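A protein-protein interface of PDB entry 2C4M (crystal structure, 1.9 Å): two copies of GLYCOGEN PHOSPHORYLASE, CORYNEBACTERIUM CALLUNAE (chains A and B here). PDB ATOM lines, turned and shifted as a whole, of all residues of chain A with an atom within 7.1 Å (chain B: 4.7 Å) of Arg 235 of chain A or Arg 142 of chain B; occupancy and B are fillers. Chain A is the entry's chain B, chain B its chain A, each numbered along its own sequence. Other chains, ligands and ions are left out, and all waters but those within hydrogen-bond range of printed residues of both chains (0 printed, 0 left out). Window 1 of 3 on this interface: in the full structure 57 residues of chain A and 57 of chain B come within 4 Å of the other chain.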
ATOM      1  N   ARG A 142       2.873  -8.925 -16.493  1.00  0.00           N
ATOM      2  CA  ARG A 142       1.807  -8.749 -17.463  1.00  0.00           C
ATOM      3  C   ARG A 142       1.672  -7.340 -18.013  1.00  0.00           C
ATOM      4  O   ARG A 142       1.412  -7.155 -19.201  1.00  0.00           O
ATOM      5  CB  ARG A 142       0.484  -9.182 -16.832  1.00  0.00           C
ATOM      6  CG  ARG A 142      -0.693  -9.115 -17.772  1.00  0.00           C
ATOM      7  CD  ARG A 142      -1.923  -9.777 -17.162  1.00  0.00           C
ATOM      8  NE  ARG A 142      -3.056  -9.716 -18.082  1.00  0.00           N
ATOM      9  CZ  ARG A 142      -4.290 -10.101 -17.770  1.00  0.00           C
ATOM     10  NH1 ARG A 142      -4.550 -10.575 -16.559  1.00  0.00           N
ATOM     11  NH2 ARG A 142      -5.264 -10.000 -18.665  1.00  0.00           N
ATOM     12  N   LYS A 211       4.492 -17.322 -13.951  1.00  0.00           N
ATOM     13  CA  LYS A 211       3.231 -16.615 -13.812  1.00  0.00           C
ATOM     14  C   LYS A 211       2.499 -17.135 -12.579  1.00  0.00           C
ATOM     15  O   LYS A 211       2.326 -18.335 -12.410  1.00  0.00           O
ATOM     16  CB  LYS A 211       2.348 -16.802 -15.046  1.00  0.00           C
ATOM     17  CG  LYS A 211       1.046 -15.998 -14.955  1.00  0.00           C
ATOM     18  CD  LYS A 211       0.125 -16.240 -16.151  1.00  0.00           C
ATOM     19  CE  LYS A 211      -1.255 -15.636 -15.877  1.00  0.00           C
ATOM     20  NZ  LYS A 211      -2.207 -15.927 -16.969  1.00  0.00           N
ATOM     21  N   ALA A 212       2.063 -16.231 -11.714  1.00  0.00           N
ATOM     22  CA  ALA A 212       1.345 -16.649 -10.517  1.00  0.00           C
ATOM     23  C   ALA A 212      -0.147 -16.725 -10.820  1.00  0.00           C
ATOM     24  O   ALA A 212      -0.718 -15.782 -11.360  1.00  0.00           O
ATOM     25  CB  ALA A 212       1.591 -15.654  -9.382  1.00  0.00           C
ATOM     26  N   GLU A 213      -0.768 -17.859 -10.511  1.00  0.00           N
ATOM     27  CA  GLU A 213      -2.198 -17.998 -10.713  1.00  0.00           C
ATOM     28  C   GLU A 213      -2.803 -18.481  -9.408  1.00  0.00           C
ATOM     29  O   GLU A 213      -2.148 -19.164  -8.618  1.00  0.00           O
ATOM     30  CB  GLU A 213      -2.510 -18.957 -11.875  1.00  0.00           C
ATOM     31  CG  GLU A 213      -2.031 -18.390 -13.213  1.00  0.00           C
ATOM     32  CD  GLU A 213      -2.493 -19.179 -14.435  1.00  0.00           C
ATOM     33  OE1 GLU A 213      -2.868 -20.358 -14.289  1.00  0.00           O
ATOM     34  OE2 GLU A 213      -2.453 -18.615 -15.554  1.00  0.00           O
ATOM     35  N   PRO A 214      -4.063 -18.114  -9.152  1.00  0.00           N
ATOM     36  CA  PRO A 214      -4.701 -18.539  -7.902  1.00  0.00           C
ATOM     37  C   PRO A 214      -4.991 -20.031  -7.809  1.00  0.00           C
ATOM     38  O   PRO A 214      -5.070 -20.725  -8.825  1.00  0.00           O
ATOM     39  CB  PRO A 214      -5.961 -17.685  -7.851  1.00  0.00           C
ATOM     40  CG  PRO A 214      -6.298 -17.487  -9.298  1.00  0.00           C
ATOM     41  CD  PRO A 214      -4.944 -17.231  -9.934  1.00  0.00           C
ATOM     42  N   GLU A 216      -7.769 -21.285  -6.588  1.00  0.00           N
ATOM     43  CA  GLU A 216      -9.152 -21.345  -7.076  1.00  0.00           C
ATOM     44  C   GLU A 216      -9.297 -20.119  -7.976  1.00  0.00           C
ATOM     45  O   GLU A 216      -8.732 -19.069  -7.664  1.00  0.00           O
ATOM     46  CB  GLU A 216     -10.159 -21.229  -5.923  1.00  0.00           C
ATOM     47  CG  GLU A 216     -10.168 -22.383  -4.936  1.00  0.00           C
ATOM     48  CD  GLU A 216     -10.906 -23.594  -5.468  1.00  0.00           C
ATOM     49  OE1 GLU A 216     -11.265 -23.593  -6.669  1.00  0.00           O
ATOM     50  OE2 GLU A 216     -11.135 -24.547  -4.684  1.00  0.00           O
ATOM     51  N   GLU A 217     -10.041 -20.238  -9.074  1.00  0.00           N
ATOM     52  CA  GLU A 217     -10.222 -19.118 -10.000  1.00  0.00           C
ATOM     53  C   GLU A 217     -10.773 -17.883  -9.316  1.00  0.00           C
ATOM     54  O   GLU A 217     -10.316 -16.773  -9.568  1.00  0.00           O
ATOM     55  CB  GLU A 217     -11.141 -19.511 -11.159  1.00  0.00           C
ATOM     56  CG  GLU A 217     -10.584 -20.617 -12.029  1.00  0.00           C
ATOM     57  CD  GLU A 217      -9.249 -20.249 -12.644  1.00  0.00           C
ATOM     58  OE1 GLU A 217      -9.096 -19.103 -13.128  1.00  0.00           O
ATOM     59  OE2 GLU A 217      -8.348 -21.116 -12.641  1.00  0.00           O
ATOM     60  N   PHE A 218     -11.786 -18.088  -8.478  1.00  0.00           N
ATOM     61  CA  PHE A 218     -12.398 -17.017  -7.704  1.00  0.00           C
ATOM     62  C   PHE A 218     -13.274 -17.687  -6.652  1.00  0.00           C
ATOM     63  O   PHE A 218     -13.520 -18.887  -6.732  1.00  0.00           O
ATOM     64  CB  PHE A 218     -13.203 -16.045  -8.598  1.00  0.00           C
ATOM     65  CG  PHE A 218     -14.336 -16.681  -9.370  1.00  0.00           C
ATOM     66  CD1 PHE A 218     -15.614 -16.766  -8.818  1.00  0.00           C
ATOM     67  CD2 PHE A 218     -14.131 -17.157 -10.662  1.00  0.00           C
ATOM     68  CE1 PHE A 218     -16.680 -17.319  -9.552  1.00  0.00           C
ATOM     69  CE2 PHE A 218     -15.185 -17.710 -11.403  1.00  0.00           C
ATOM     70  CZ  PHE A 218     -16.461 -17.790 -10.843  1.00  0.00           C
ATOM     71  N   ASP A 219     -13.703 -16.926  -5.654  1.00  0.00           N
ATOM     72  CA  ASP A 219     -14.538 -17.454  -4.575  1.00  0.00           C
ATOM     73  C   ASP A 219     -15.956 -17.610  -5.121  1.00  0.00           C
ATOM     74  O   ASP A 219     -16.727 -16.652  -5.114  1.00  0.00           O
ATOM     75  CB  ASP A 219     -14.537 -16.463  -3.412  1.00  0.00           C
ATOM     76  CG  ASP A 219     -15.149 -17.036  -2.150  1.00  0.00           C
ATOM     77  OD1 ASP A 219     -16.086 -17.856  -2.259  1.00  0.00           O
ATOM     78  OD2 ASP A 219     -14.698 -16.646  -1.049  1.00  0.00           O
ATOM     79  N   ASP A 230     -15.738  -9.105  -3.252  1.00  0.00           N
ATOM     80  CA  ASP A 230     -15.165 -10.081  -2.335  1.00  0.00           C
ATOM     81  C   ASP A 230     -14.771 -11.355  -3.076  1.00  0.00           C
ATOM     82  O   ASP A 230     -13.768 -11.990  -2.755  1.00  0.00           O
ATOM     83  CB  ASP A 230     -16.168 -10.465  -1.245  1.00  0.00           C
ATOM     84  CG  ASP A 230     -16.445  -9.335  -0.273  1.00  0.00           C
ATOM     85  OD1 ASP A 230     -15.773  -8.280  -0.355  1.00  0.00           O
ATOM     86  OD2 ASP A 230     -17.342  -9.507   0.580  1.00  0.00           O
ATOM     87  N   ALA A 231     -15.571 -11.734  -4.070  1.00  0.00           N
ATOM     88  CA  ALA A 231     -15.333 -12.973  -4.829  1.00  0.00           C
ATOM     89  C   ALA A 231     -13.985 -12.997  -5.568  1.00  0.00           C
ATOM     90  O   ALA A 231     -13.446 -14.061  -5.858  1.00  0.00           O
ATOM     91  CB  ALA A 231     -16.476 -13.193  -5.803  1.00  0.00           C
ATOM     92  N   ILE A 232     -13.457 -11.799  -5.926  1.00  0.00           N
ATOM     93  CA  ILE A 232     -12.195 -11.779  -6.670  1.00  0.00           C
ATOM     94  C   ILE A 232     -11.010 -11.159  -5.901  1.00  0.00           C
ATOM     95  O   ILE A 232      -9.925 -10.997  -6.448  1.00  0.00           O
ATOM     96  CB  ILE A 232     -12.395 -11.040  -7.999  1.00  0.00           C
ATOM     97  CG1 ILE A 232     -13.075  -9.687  -7.772  1.00  0.00           C
ATOM     98  CG2 ILE A 232     -13.279 -11.867  -8.951  1.00  0.00           C
ATOM     99  CD1 ILE A 232     -12.145  -8.672  -7.107  1.00  0.00           C
ATOM    100  N   ILE A 233     -11.209 -10.763  -4.617  1.00  0.00           N
ATOM    101  CA  ILE A 233     -10.083 -10.120  -3.929  1.00  0.00           C
ATOM    102  C   ILE A 233      -8.838 -11.009  -3.916  1.00  0.00           C
ATOM    103  O   ILE A 233      -7.730 -10.578  -4.202  1.00  0.00           O
ATOM    104  CB  ILE A 233     -10.489  -9.775  -2.487  1.00  0.00           C
ATOM    105  CG1 ILE A 233     -11.404  -8.546  -2.461  1.00  0.00           C
ATOM    106  CG2 ILE A 233      -9.237  -9.424  -1.668  1.00  0.00           C
ATOM    107  CD1 ILE A 233     -12.012  -8.295  -1.080  1.00  0.00           C
ATOM    108  N   GLU A 234      -9.043 -12.273  -3.499  1.00  0.00           N
ATOM    109  CA  GLU A 234      -7.896 -13.165  -3.419  1.00  0.00           C
ATOM    110  C   GLU A 234      -7.321 -13.464  -4.808  1.00  0.00           C
ATOM    111  O   GLU A 234      -6.115 -13.554  -5.004  1.00  0.00           O
ATOM    112  CB  GLU A 234      -8.328 -14.464  -2.731  1.00  0.00           C
ATOM    113  CG  GLU A 234      -8.644 -14.271  -1.249  1.00  0.00           C
ATOM    114  CD  GLU A 234      -7.491 -13.567  -0.566  1.00  0.00           C
ATOM    115  OE1 GLU A 234      -6.376 -14.085  -0.610  1.00  0.00           O
ATOM    116  OE2 GLU A 234      -7.713 -12.518   0.026  1.00  0.00           O
ATOM    117  N   ARG A 235      -8.169 -13.616  -5.820  1.00  0.00           N
ATOM    118  CA  ARG A 235      -7.671 -13.851  -7.172  1.00  0.00           C
ATOM    119  C   ARG A 235      -6.760 -12.707  -7.599  1.00  0.00           C
ATOM    120  O   ARG A 235      -5.679 -12.938  -8.152  1.00  0.00           O
ATOM    121  CB  ARG A 235      -8.824 -13.947  -8.177  1.00  0.00           C
ATOM    122  CG  ARG A 235      -8.356 -13.990  -9.627  1.00  0.00           C
ATOM    123  CD  ARG A 235      -9.522 -13.839 -10.590  1.00  0.00           C
ATOM    124  NE  ARG A 235      -9.093 -13.925 -11.982  1.00  0.00           N
ATOM    125  CZ  ARG A 235      -8.763 -15.061 -12.594  1.00  0.00           C
ATOM    126  NH1 ARG A 235      -8.823 -16.206 -11.930  1.00  0.00           N
ATOM    127  NH2 ARG A 235      -8.363 -15.049 -13.862  1.00  0.00           N
ATOM    128  N   GLU A 236      -7.178 -11.473  -7.331  1.00  0.00           N
ATOM    129  CA  GLU A 236      -6.370 -10.339  -7.749  1.00  0.00           C
ATOM    130  C   GLU A 236      -5.144 -10.096  -6.865  1.00  0.00           C
ATOM    131  O   GLU A 236      -4.171  -9.503  -7.322  1.00  0.00           O
ATOM    132  CB  GLU A 236      -7.235  -9.079  -7.868  1.00  0.00           C
ATOM    133  CG  GLU A 236      -8.355  -9.243  -8.908  1.00  0.00           C
ATOM    134  CD  GLU A 236      -7.833  -9.645 -10.286  1.00  0.00           C
ATOM    135  OE1 GLU A 236      -6.790  -9.106 -10.721  1.00  0.00           O
ATOM    136  OE2 GLU A 236      -8.473 -10.495 -10.945  1.00  0.00           O
ATOM    137  N   ARG A 237      -5.180 -10.553  -5.617  1.00  0.00           N
ATOM    138  CA  ARG A 237      -4.014 -10.399  -4.752  1.00  0.00           C
ATOM    139  C   ARG A 237      -2.912 -11.288  -5.344  1.00  0.00           C
ATOM    140  O   ARG A 237      -1.746 -10.908  -5.388  1.00  0.00           O
ATOM    141  CB  ARG A 237      -4.327 -10.822  -3.310  1.00  0.00           C
ATOM    142  CG  ARG A 237      -5.037  -9.752  -2.484  1.00  0.00           C
ATOM    143  CD  ARG A 237      -5.713 -10.373  -1.268  1.00  0.00           C
ATOM    144  NE  ARG A 237      -4.776 -11.143  -0.458  1.00  0.00           N
ATOM    145  CZ  ARG A 237      -3.751 -10.622   0.213  1.00  0.00           C
ATOM    146  NH1 ARG A 237      -3.516  -9.312   0.174  1.00  0.00           N
ATOM    147  NH2 ARG A 237      -2.952 -11.416   0.926  1.00  0.00           N
ATOM    148  N   VAL A 238      -3.294 -12.474  -5.812  1.00  0.00           N
ATOM    149  CA  VAL A 238      -2.328 -13.381  -6.424  1.00  0.00           C
ATOM    150  C   VAL A 238      -1.837 -12.786  -7.744  1.00  0.00           C
ATOM    151  O   VAL A 238      -0.644 -12.830  -8.052  1.00  0.00           O
ATOM    152  CB  VAL A 238      -2.951 -14.765  -6.675  1.00  0.00           C
ATOM    153  CG1 VAL A 238      -1.984 -15.650  -7.471  1.00  0.00           C
ATOM    154  CG2 VAL A 238      -3.292 -15.414  -5.352  1.00  0.00           C
ATOM    155  N   SER A 239      -2.761 -12.230  -8.522  1.00  0.00           N
ATOM    156  CA  SER A 239      -2.425 -11.607  -9.799  1.00  0.00           C
ATOM    157  C   SER A 239      -1.465 -10.424  -9.627  1.00  0.00           C
ATOM    158  O   SER A 239      -0.680 -10.115 -10.519  1.00  0.00           O
ATOM    159  CB  SER A 239      -3.692 -11.109 -10.498  1.00  0.00           C
ATOM    160  OG  SER A 239      -4.526 -12.187 -10.882  1.00  0.00           O
ATOM    161  N   ASP A 240      -1.550  -9.746  -8.493  1.00  0.00           N
ATOM    162  CA  ASP A 240      -0.673  -8.606  -8.239  1.00  0.00           C
ATOM    163  C   ASP A 240       0.802  -9.020  -8.283  1.00  0.00           C
ATOM    164  O   ASP A 240       1.678  -8.203  -8.546  1.00  0.00           O
ATOM    165  CB  ASP A 240      -1.017  -7.982  -6.890  1.00  0.00           C
ATOM    166  CG  ASP A 240      -2.281  -7.154  -6.944  1.00  0.00           C
ATOM    167  OD1 ASP A 240      -2.656  -6.698  -8.048  1.00  0.00           O
ATOM    168  OD2 ASP A 240      -2.904  -6.960  -5.878  1.00  0.00           O
ATOM    169  N   ARG A 243       1.534  -8.490 -11.935  1.00  0.00           N
ATOM    170  CA  ARG A 243       0.881  -7.376 -12.613  1.00  0.00           C
ATOM    171  C   ARG A 243       1.825  -6.305 -13.125  1.00  0.00           C
ATOM    172  O   ARG A 243       1.827  -5.981 -14.315  1.00  0.00           O
ATOM    173  CB  ARG A 243      -0.165  -6.720 -11.696  1.00  0.00           C
ATOM    174  CG  ARG A 243      -1.181  -5.837 -12.438  1.00  0.00           C
ATOM    175  CD  ARG A 243      -2.158  -5.149 -11.475  1.00  0.00           C
ATOM    176  NE  ARG A 243      -2.861  -6.106 -10.621  1.00  0.00           N
ATOM    177  CZ  ARG A 243      -3.889  -6.854 -11.005  1.00  0.00           C
ATOM    178  NH1 ARG A 243      -4.361  -6.760 -12.249  1.00  0.00           N
ATOM    179  NH2 ARG A 243      -4.443  -7.699 -10.140  1.00  0.00           N
ATOM    180  N   LEU B 140     -19.171 -14.635 -24.478  1.00  0.00           N
ATOM    181  CA  LEU B 140     -18.064 -15.568 -24.307  1.00  0.00           C
ATOM    182  C   LEU B 140     -17.868 -15.741 -22.809  1.00  0.00           C
ATOM    183  O   LEU B 140     -16.993 -15.103 -22.214  1.00  0.00           O
ATOM    184  CB  LEU B 140     -16.773 -15.021 -24.936  1.00  0.00           C
ATOM    185  CG  LEU B 140     -15.543 -15.943 -24.880  1.00  0.00           C
ATOM    186  CD1 LEU B 140     -15.703 -17.048 -25.898  1.00  0.00           C
ATOM    187  CD2 LEU B 140     -14.277 -15.166 -25.200  1.00  0.00           C
ATOM    188  N   TYR B 141     -18.690 -16.588 -22.188  1.00  0.00           N
ATOM    189  CA  TYR B 141     -18.584 -16.824 -20.749  1.00  0.00           C
ATOM    190  C   TYR B 141     -17.253 -17.502 -20.445  1.00  0.00           C
ATOM    191  O   TYR B 141     -16.904 -18.520 -21.043  1.00  0.00           O
ATOM    192  CB  TYR B 141     -19.738 -17.691 -20.251  1.00  0.00           C
ATOM    193  CG  TYR B 141     -21.104 -17.096 -20.507  1.00  0.00           C
ATOM    194  CD1 TYR B 141     -21.560 -16.045 -19.717  1.00  0.00           C
ATOM    195  CD2 TYR B 141     -21.920 -17.607 -21.516  1.00  0.00           C
ATOM    196  CE1 TYR B 141     -22.818 -15.503 -19.937  1.00  0.00           C
ATOM    197  CE2 TYR B 141     -23.181 -17.072 -21.730  1.00  0.00           C
ATOM    198  CZ  TYR B 141     -23.632 -16.028 -20.943  1.00  0.00           C
ATOM    199  OH  TYR B 141     -24.875 -15.471 -21.168  1.00  0.00           O
ATOM    200  N   ARG B 142     -16.508 -16.939 -19.509  1.00  0.00           N
ATOM    201  CA  ARG B 142     -15.189 -17.494 -19.212  1.00  0.00           C
ATOM    202  C   ARG B 142     -15.254 -18.732 -18.318  1.00  0.00           C
ATOM    203  O   ARG B 142     -14.524 -19.698 -18.502  1.00  0.00           O
ATOM    204  CB  ARG B 142     -14.395 -16.409 -18.509  1.00  0.00           C
ATOM    205  CG  ARG B 142     -13.012 -16.884 -18.112  1.00  0.00           C
ATOM    206  CD  ARG B 142     -12.074 -15.703 -17.929  1.00  0.00           C
ATOM    207  NE  ARG B 142     -10.716 -16.186 -17.761  1.00  0.00           N
ATOM    208  CZ  ARG B 142      -9.822 -15.314 -17.272  1.00  0.00           C
ATOM    209  NH1 ARG B 142     -10.188 -14.084 -16.958  1.00  0.00           N
ATOM    210  NH2 ARG B 142      -8.563 -15.714 -17.069  1.00  0.00           N
ATOM    211  N   PHE B 143     -16.162 -18.749 -17.340  1.00  0.00           N
ATOM    212  CA  PHE B 143     -16.270 -19.872 -16.404  1.00  0.00           C
ATOM    213  C   PHE B 143     -17.607 -20.631 -16.371  1.00  0.00           C
ATOM    214  O   PHE B 143     -17.934 -21.259 -15.370  1.00  0.00           O
ATOM    215  CB  PHE B 143     -15.921 -19.370 -14.998  1.00  0.00           C
ATOM    216  CG  PHE B 143     -14.545 -18.745 -14.899  1.00  0.00           C
ATOM    217  CD1 PHE B 143     -13.405 -19.541 -14.870  1.00  0.00           C
ATOM    218  CD2 PHE B 143     -14.394 -17.362 -14.823  1.00  0.00           C
ATOM    219  CE1 PHE B 143     -12.130 -18.974 -14.761  1.00  0.00           C
ATOM    220  CE2 PHE B 143     -13.117 -16.778 -14.713  1.00  0.00           C
ATOM    221  CZ  PHE B 143     -11.987 -17.586 -14.682  1.00  0.00           C
ATOM    222  N   GLY B 144     -18.372 -20.568 -17.462  1.00  0.00           N
ATOM    223  CA  GLY B 144     -19.639 -21.299 -17.580  1.00  0.00           C
ATOM    224  C   GLY B 144     -20.616 -21.040 -16.426  1.00  0.00           C
ATOM    225  O   GLY B 144     -20.727 -19.943 -15.896  1.00  0.00           O
ATOM    226  N   ASP B 160     -15.965 -23.047 -13.755  1.00  0.00           N
ATOM    227  CA  ASP B 160     -15.848 -24.052 -14.818  1.00  0.00           C
ATOM    228  C   ASP B 160     -15.032 -23.496 -15.988  1.00  0.00           C
ATOM    229  O   ASP B 160     -15.570 -23.210 -17.051  1.00  0.00           O
ATOM    230  CB  ASP B 160     -17.253 -24.469 -15.288  1.00  0.00           C
ATOM    231  CG  ASP B 160     -17.237 -25.702 -16.184  1.00  0.00           C
ATOM    232  OD1 ASP B 160     -16.250 -26.471 -16.147  1.00  0.00           O
ATOM    233  OD2 ASP B 160     -18.228 -25.910 -16.916  1.00  0.00           O
ATOM    234  N   PRO B 161     -13.711 -23.337 -15.798  1.00  0.00           N
ATOM    235  CA  PRO B 161     -12.860 -22.805 -16.867  1.00  0.00           C
ATOM    236  C   PRO B 161     -12.795 -23.750 -18.057  1.00  0.00           C
ATOM    237  O   PRO B 161     -12.932 -24.962 -17.897  1.00  0.00           O
ATOM    238  CB  PRO B 161     -11.504 -22.648 -16.179  1.00  0.00           C
ATOM    239  CG  PRO B 161     -11.455 -23.699 -15.114  1.00  0.00           C
ATOM    240  CD  PRO B 161     -12.902 -23.707 -14.621  1.00  0.00           C
ATOM    241  N   TRP B 162     -12.579 -23.198 -19.246  1.00  0.00           N
ATOM    242  CA  TRP B 162     -12.498 -24.021 -20.447  1.00  0.00           C
ATOM    243  C   TRP B 162     -11.558 -23.430 -21.489  1.00  0.00           C
ATOM    244  O   TRP B 162     -11.071 -24.144 -22.356  1.00  0.00           O
ATOM    245  CB  TRP B 162     -13.892 -24.212 -21.070  1.00  0.00           C
ATOM    246  CG  TRP B 162     -14.533 -22.940 -21.509  1.00  0.00           C
ATOM    247  CD1 TRP B 162     -15.162 -22.026 -20.717  1.00  0.00           C
ATOM    248  CD2 TRP B 162     -14.565 -22.408 -22.841  1.00  0.00           C
ATOM    249  NE1 TRP B 162     -15.583 -20.954 -21.469  1.00  0.00           N
ATOM    250  CE2 TRP B 162     -15.229 -21.162 -22.777  1.00  0.00           C
ATOM    251  CE3 TRP B 162     -14.095 -22.862 -24.083  1.00  0.00           C
ATOM    252  CZ2 TRP B 162     -15.436 -20.360 -23.906  1.00  0.00           C
ATOM    253  CZ3 TRP B 162     -14.298 -22.069 -25.206  1.00  0.00           C
ATOM    254  CH2 TRP B 162     -14.966 -20.828 -25.110  1.00  0.00           C
ATOM    255  N   GLU B 164      -8.808 -21.263 -20.582  1.00  0.00           N
ATOM    256  CA  GLU B 164      -7.679 -20.656 -19.895  1.00  0.00           C
ATOM    257  C   GLU B 164      -6.414 -20.996 -20.678  1.00  0.00           C
ATOM    258  O   GLU B 164      -5.417 -20.278 -20.617  1.00  0.00           O
ATOM    259  CB  GLU B 164      -7.582 -21.176 -18.465  1.00  0.00           C
ATOM    260  CG  GLU B 164      -8.754 -20.733 -17.598  1.00  0.00           C
ATOM    261  CD  GLU B 164      -8.976 -19.228 -17.652  1.00  0.00           C
ATOM    262  OE1 GLU B 164      -8.060 -18.470 -17.253  1.00  0.00           O
ATOM    263  OE2 GLU B 164     -10.071 -18.801 -18.084  1.00  0.00           O
ATOM    264  N   CYS B 242     -18.719 -11.204 -18.358  1.00  0.00           N
ATOM    265  CA  CYS B 242     -18.505 -12.498 -19.030  1.00  0.00           C
ATOM    266  C   CYS B 242     -17.999 -13.613 -18.088  1.00  0.00           C
ATOM    267  O   CYS B 242     -17.632 -14.701 -18.512  1.00  0.00           O
ATOM    268  CB  CYS B 242     -17.504 -12.285 -20.165  1.00  0.00           C
ATOM    269  SG  CYS B 242     -18.196 -11.301 -21.513  1.00  0.00           S
ATOM    270  N   ARG B 243     -18.018 -13.356 -16.754  1.00  0.00           N
ATOM    271  CA  ARG B 243     -17.424 -14.338 -15.840  1.00  0.00           C
ATOM    272  C   ARG B 243     -18.188 -15.672 -15.796  1.00  0.00           C
ATOM    273  O   ARG B 243     -17.654 -16.731 -16.111  1.00  0.00           O
ATOM    274  CB  ARG B 243     -17.327 -13.741 -14.435  1.00  0.00           C
ATOM    275  CG  ARG B 243     -16.679 -14.719 -13.453  1.00  0.00           C
ATOM    276  CD  ARG B 243     -16.383 -14.083 -12.090  1.00  0.00           C
ATOM    277  NE  ARG B 243     -16.177 -12.640 -12.224  1.00  0.00           N
ATOM    278  CZ  ARG B 243     -14.909 -12.202 -12.338  1.00  0.00           C
ATOM    279  NH1 ARG B 243     -13.906 -13.064 -12.356  1.00  0.00           N
ATOM    280  NH2 ARG B 243     -14.670 -10.890 -12.425  1.00  0.00           N
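NH2 of Arg 235 of chain A sits close to NH2 of Arg 142 of chain B (3.3 Å).
Printed residues of chain B that touch a printed residue of chain A: Arg 142, Phe 143 and Arg 243. Hydrophobic or aromatic side chains of chain B within 4 Å of the printed part of chain A: Phe 143. Along chain B the printed residues that touch a printed residue of chain A span positions 142 to 243. Of the 21 printed residues of chain A, 4 touch a printed residue of chain B. Among the printed residues, 5 pairs touch across the chains.
The backbone NH (N) of Phe 143 of chain B is in hydrogen-bond range of the backbone carbonyl oxygen (O) of Arg 243 of chain B, 2.8 Å away. The guanidinium group (NE) of Arg 235 of chain A is in salt-bridge range of the side-chain carboxylate (OE2) of Glu 236 of chain A, at 3.6 Å. O of Cys 242 of chain B lies within hydrogen-bond range of N of Arg 142 of chain B. The backbone carbonyl oxygen of Phe 143 of chain B lies within hydrogen-bond range of the backbone NH of Asp 160 of chain B, at 3.1 Å. The backbone carbonyl oxygen (O) of Arg 142 of chain B sits close to the indole nitrogen (NE1) of Trp 162 of chain B, at 3.4 Å. OE2 of Glu 164 of chain B is in salt-bridge range of NE of Arg 142 of chain B, 2.7 Å away.
2 positions are printed for both chains. Of the 5 pairs that touch across the chains among the printed residues, none has its exchanged pair printed and touching as well.
Of chain B, only Arg 142 comes within 4 Å of Arg 235 of chain A. Printed residues of chain B within 4 Å of Phe 218 of chain A: Phe 143 (3.5 Å) and Arg 243 (3.9 Å). Of the printed residues of chain A, Phe 143 of chain B touches Glu 217 and Phe 218. Of the printed residues of chain A, Arg 243 of chain B touches Phe 218 (3.9 Å) and Ile 232 (3.7 Å). Printed residues of chain B within 4 Å of Ile 232 of chain A: Arg 243 (3.7 Å). Of the printed residues of chain B, Glu 217 of chain A touches Phe 143 (3.4 Å). Arg 237 of chain A touches none of the printed residues of chain B. The nearest residue of chain B that does not touch Arg 235 of chain A is Phe 143 of chain B (4.4 Å).
Glu 217 of chain A touches Phe 143 of chain B (OE1 to CE1, 3.4 Å). Phe 143 of chain B touches Phe 218 of chain A (CD2 to CE2, 3.5 Å). Phe 218 of chain A touches Arg 243 of chain B (CE2 to CD, 3.9 Å). Arg 243 of chain B touches Ile 232 of chain A (NH1 to CG2, 3.7 Å).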
